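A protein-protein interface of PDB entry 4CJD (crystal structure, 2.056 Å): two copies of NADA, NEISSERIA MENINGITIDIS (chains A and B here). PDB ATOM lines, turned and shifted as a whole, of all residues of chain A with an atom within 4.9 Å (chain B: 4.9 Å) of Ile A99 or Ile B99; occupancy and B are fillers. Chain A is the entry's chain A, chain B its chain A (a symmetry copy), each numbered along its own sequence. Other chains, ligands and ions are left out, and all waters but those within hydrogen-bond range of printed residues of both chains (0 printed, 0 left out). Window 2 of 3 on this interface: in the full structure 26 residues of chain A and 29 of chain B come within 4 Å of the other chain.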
ATOM      1  N   VAL A  95       5.735  24.686  23.520  1.00  0.00           N
ATOM      2  CA  VAL A  95       5.798  23.369  24.133  1.00  0.00           C
ATOM      3  C   VAL A  95       4.408  22.938  24.604  1.00  0.00           C
ATOM      4  O   VAL A  95       3.992  21.796  24.375  1.00  0.00           O
ATOM      5  CB  VAL A  95       6.778  23.335  25.317  1.00  0.00           C
ATOM      6  CG1 VAL A  95       6.574  22.081  26.137  1.00  0.00           C
ATOM      7  CG2 VAL A  95       8.208  23.420  24.825  1.00  0.00           C
ATOM      8  N   VAL A  96       3.677  23.861  25.223  1.00  0.00           N
ATOM      9  CA  VAL A  96       2.369  23.522  25.778  1.00  0.00           C
ATOM     10  C   VAL A  96       1.385  23.126  24.676  1.00  0.00           C
ATOM     11  O   VAL A  96       0.626  22.176  24.833  1.00  0.00           O
ATOM     12  CB  VAL A  96       1.787  24.689  26.607  1.00  0.00           C
ATOM     13  CG1 VAL A  96       0.314  24.430  26.923  1.00  0.00           C
ATOM     14  CG2 VAL A  96       2.598  24.882  27.890  1.00  0.00           C
ATOM     15  N   ASN A  97       1.413  23.843  23.558  1.00  0.00           N
ATOM     16  CA  ASN A  97       0.552  23.510  22.437  1.00  0.00           C
ATOM     17  C   ASN A  97       0.883  22.112  21.910  1.00  0.00           C
ATOM     18  O   ASN A  97      -0.016  21.297  21.659  1.00  0.00           O
ATOM     19  CB  ASN A  97       0.680  24.558  21.330  1.00  0.00           C
ATOM     20  CG  ASN A  97       0.150  25.930  21.754  1.00  0.00           C
ATOM     21  OD1 ASN A  97      -0.756  26.031  22.582  1.00  0.00           O
ATOM     22  ND2 ASN A  97       0.719  26.990  21.188  1.00  0.00           N
ATOM     23  N   ASP A  98       2.180  21.839  21.773  1.00  0.00           N
ATOM     24  CA  ASP A  98       2.664  20.512  21.405  1.00  0.00           C
ATOM     25  C   ASP A  98       2.113  19.442  22.335  1.00  0.00           C
ATOM     26  O   ASP A  98       1.624  18.398  21.886  1.00  0.00           O
ATOM     27  CB  ASP A  98       4.190  20.469  21.437  1.00  0.00           C
ATOM     28  CG  ASP A  98       4.812  21.192  20.275  1.00  0.00           C
ATOM     29  OD1 ASP A  98       4.070  21.517  19.324  1.00  0.00           O
ATOM     30  OD2 ASP A  98       6.042  21.423  20.309  1.00  0.00           O
ATOM     31  N   ILE A  99       2.203  19.697  23.636  1.00  0.00           N
ATOM     32  CA  ILE A  99       1.705  18.741  24.609  1.00  0.00           C
ATOM     33  C   ILE A  99       0.190  18.620  24.480  1.00  0.00           C
ATOM     34  O   ILE A  99      -0.365  17.539  24.642  1.00  0.00           O
ATOM     35  CB  ILE A  99       2.098  19.140  26.042  1.00  0.00           C
ATOM     36  CG1 ILE A  99       3.606  18.997  26.225  1.00  0.00           C
ATOM     37  CG2 ILE A  99       1.382  18.263  27.071  1.00  0.00           C
ATOM     38  CD1 ILE A  99       4.083  19.345  27.620  1.00  0.00           C
ATOM     39  N   SER A 100      -0.472  19.725  24.154  1.00  0.00           N
ATOM     40  CA  SER A 100      -1.921  19.719  24.015  1.00  0.00           C
ATOM     41  C   SER A 100      -2.364  18.845  22.834  1.00  0.00           C
ATOM     42  O   SER A 100      -3.448  18.261  22.850  1.00  0.00           O
ATOM     43  CB  SER A 100      -2.450  21.144  23.855  1.00  0.00           C
ATOM     44  OG  SER A 100      -3.835  21.203  24.157  1.00  0.00           O
ATOM     45  N   ALA A 101      -1.521  18.748  21.815  1.00  0.00           N
ATOM     46  CA  ALA A 101      -1.824  17.901  20.667  1.00  0.00           C
ATOM     47  C   ALA A 101      -1.616  16.429  21.015  1.00  0.00           C
ATOM     48  O   ALA A 101      -2.381  15.542  20.576  1.00  0.00           O
ATOM     49  CB  ALA A 101      -0.963  18.296  19.477  1.00  0.00           C
ATOM     50  N   ASP A 102      -0.580  16.166  21.807  1.00  0.00           N
ATOM     51  CA  ASP A 102      -0.266  14.796  22.200  1.00  0.00           C
ATOM     52  C   ASP A 102      -1.288  14.246  23.194  1.00  0.00           C
ATOM     53  O   ASP A 102      -1.601  13.056  23.167  1.00  0.00           O
ATOM     54  CB  ASP A 102       1.145  14.709  22.786  1.00  0.00           C
ATOM     55  CG  ASP A 102       2.215  15.095  21.783  1.00  0.00           C
ATOM     56  OD1 ASP A 102       1.966  14.957  20.567  1.00  0.00           O
ATOM     57  OD2 ASP A 102       3.305  15.539  22.209  1.00  0.00           O
ATOM     58  N   VAL A 103      -1.819  15.099  24.065  1.00  0.00           N
ATOM     59  CA  VAL A 103      -2.809  14.627  25.029  1.00  0.00           C
ATOM     60  C   VAL A 103      -4.126  14.300  24.328  1.00  0.00           C
ATOM     61  O   VAL A 103      -4.860  13.418  24.763  1.00  0.00           O
ATOM     62  CB  VAL A 103      -3.049  15.651  26.162  1.00  0.00           C
ATOM     63  CG1 VAL A 103      -3.577  16.947  25.608  1.00  0.00           C
ATOM     64  CG2 VAL A 103      -4.017  15.097  27.194  1.00  0.00           C
ATOM     65  N   VAL B  95       6.557  22.401  35.991  1.00  0.00           N
ATOM     66  CA  VAL B  95       5.326  21.643  35.842  1.00  0.00           C
ATOM     67  C   VAL B  95       5.219  21.085  34.422  1.00  0.00           C
ATOM     68  O   VAL B  95       4.880  19.911  34.230  1.00  0.00           O
ATOM     69  CB  VAL B  95       4.086  22.495  36.157  1.00  0.00           C
ATOM     70  CG1 VAL B  95       2.832  21.803  35.672  1.00  0.00           C
ATOM     71  CG2 VAL B  95       3.998  22.771  37.644  1.00  0.00           C
ATOM     72  N   VAL B  96       5.546  21.911  33.432  1.00  0.00           N
ATOM     73  CA  VAL B  96       5.400  21.495  32.039  1.00  0.00           C
ATOM     74  C   VAL B  96       6.335  20.330  31.709  1.00  0.00           C
ATOM     75  O   VAL B  96       5.941  19.393  31.023  1.00  0.00           O
ATOM     76  CB  VAL B  96       5.660  22.668  31.068  1.00  0.00           C
ATOM     77  CG1 VAL B  96       5.795  22.150  29.636  1.00  0.00           C
ATOM     78  CG2 VAL B  96       4.537  23.701  31.175  1.00  0.00           C
ATOM     79  N   ASN B  97       7.563  20.383  32.210  1.00  0.00           N
ATOM     80  CA  ASN B  97       8.505  19.298  31.992  1.00  0.00           C
ATOM     81  C   ASN B  97       7.976  18.004  32.616  1.00  0.00           C
ATOM     82  O   ASN B  97       8.011  16.935  31.987  1.00  0.00           O
ATOM     83  CB  ASN B  97       9.880  19.658  32.558  1.00  0.00           C
ATOM     84  CG  ASN B  97      10.539  20.818  31.808  1.00  0.00           C
ATOM     85  OD1 ASN B  97      10.302  21.019  30.617  1.00  0.00           O
ATOM     86  ND2 ASN B  97      11.366  21.587  32.510  1.00  0.00           N
ATOM     87  N   ASP B  98       7.466  18.119  33.840  1.00  0.00           N
ATOM     88  CA  ASP B  98       6.808  17.007  34.519  1.00  0.00           C
ATOM     89  C   ASP B  98       5.700  16.412  33.666  1.00  0.00           C
ATOM     90  O   ASP B  98       5.604  15.189  33.506  1.00  0.00           O
ATOM     91  CB  ASP B  98       6.223  17.464  35.855  1.00  0.00           C
ATOM     92  CG  ASP B  98       7.280  17.685  36.901  1.00  0.00           C
ATOM     93  OD1 ASP B  98       8.430  17.258  36.669  1.00  0.00           O
ATOM     94  OD2 ASP B  98       6.955  18.274  37.957  1.00  0.00           O
ATOM     95  N   ILE B  99       4.851  17.279  33.122  1.00  0.00           N
ATOM     96  CA  ILE B  99       3.757  16.815  32.287  1.00  0.00           C
ATOM     97  C   ILE B  99       4.316  16.180  31.018  1.00  0.00           C
ATOM     98  O   ILE B  99       3.771  15.202  30.518  1.00  0.00           O
ATOM     99  CB  ILE B  99       2.788  17.958  31.943  1.00  0.00           C
ATOM    100  CG1 ILE B  99       2.042  18.400  33.197  1.00  0.00           C
ATOM    101  CG2 ILE B  99       1.774  17.517  30.885  1.00  0.00           C
ATOM    102  CD1 ILE B  99       1.040  19.511  32.947  1.00  0.00           C
ATOM    103  N   SER B 100       5.423  16.718  30.519  1.00  0.00           N
ATOM    104  CA  SER B 100       6.031  16.194  29.304  1.00  0.00           C
ATOM    105  C   SER B 100       6.560  14.769  29.517  1.00  0.00           C
ATOM    106  O   SER B 100       6.594  13.961  28.587  1.00  0.00           O
ATOM    107  CB  SER B 100       7.153  17.115  28.825  1.00  0.00           C
ATOM    108  OG  SER B 100       7.449  16.878  27.459  1.00  0.00           O
ATOM    109  N   ALA B 101       6.962  14.458  30.742  1.00  0.00           N
ATOM    110  CA  ALA B 101       7.432  13.116  31.061  1.00  0.00           C
ATOM    111  C   ALA B 101       6.259  12.147  31.172  1.00  0.00           C
ATOM    112  O   ALA B 101       6.343  10.970  30.754  1.00  0.00           O
ATOM    113  CB  ALA B 101       8.238  13.130  32.350  1.00  0.00           C
ATOM    114  N   ASP B 102       5.158  12.639  31.733  1.00  0.00           N
ATOM    115  CA  ASP B 102       3.971  11.808  31.910  1.00  0.00           C
ATOM    116  C   ASP B 102       3.278  11.522  30.578  1.00  0.00           C
ATOM    117  O   ASP B 102       2.726  10.439  30.388  1.00  0.00           O
ATOM    118  CB  ASP B 102       2.991  12.462  32.888  1.00  0.00           C
ATOM    119  CG  ASP B 102       3.580  12.625  34.276  1.00  0.00           C
ATOM    120  OD1 ASP B 102       4.488  11.844  34.631  1.00  0.00           O
ATOM    121  OD2 ASP B 102       3.136  13.534  35.013  1.00  0.00           O
ATOM    122  N   VAL B 103       3.309  12.476  29.652  1.00  0.00           N
ATOM    123  CA  VAL B 103       2.673  12.248  28.358  1.00  0.00           C
ATOM    124  C   VAL B 103       3.467  11.230  27.541  1.00  0.00           C
ATOM    125  O   VAL B 103       2.897  10.491  26.745  1.00  0.00           O
ATOM    126  CB  VAL B 103       2.505  13.560  27.555  1.00  0.00           C
ATOM    127  CG1 VAL B 103       3.845  14.184  27.269  1.00  0.00           C
ATOM    128  CG2 VAL B 103       1.764  13.306  26.254  1.00  0.00           C
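Val A95 touches Val B96, but with the chains exchanged Val A96 does not touch Val B95 (8.0 Å).
Ile A99 touches Val B96, but with the chains exchanged Val A96 does not touch Ile B99 (7.5 Å).
Ile B99 touches its own counterpart, Ile A99.
Ile A99 touches Ser B100, but with the chains exchanged Ser A100 does not touch Ile B99 (7.4 Å).
Of the 9 printed residues of chain A, 4 touch a printed residue of chain B.
Hydrophobic or aromatic side chains of chain A that line the printed part of chain B: Val A95, Val A96 and Ile A99.
Of the 9 printed residues of chain B, 4 touch a printed residue of chain A.
Hydrophobic or aromatic side chains of chain B within 4 Å of the printed part of chain A: Val B96, Ile B99 and Val B103.
Among the printed residues, no Asp or Glu carboxylate lies within 4 Å of a Lys or Arg side-chain nitrogen of the other chain.
Among the printed residues, pairs that only touch across the chains: Val A95 with Val B96 (3.6 Å), Val A96 with Val B96 (3.99 Å), Ile A99 with Val B96 (3.9 Å), Ile A99 with Ile B99 (3.9 Å), Ile A99 with Ser B100 (3.98 Å) and Asp A102 with Val B103 (3.8 Å).
Of the printed residues of chain B, Val A96 touches Val B96.
Asn A97 touches none of the printed residues of chain B.
Ser A100 touches none of the printed residues of chain B.
Ile B99 touches just one residue of chain A: Ile A99 (3.9 Å).
Printed residues of chain A within 4 Å of Val B103: Asp A102.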
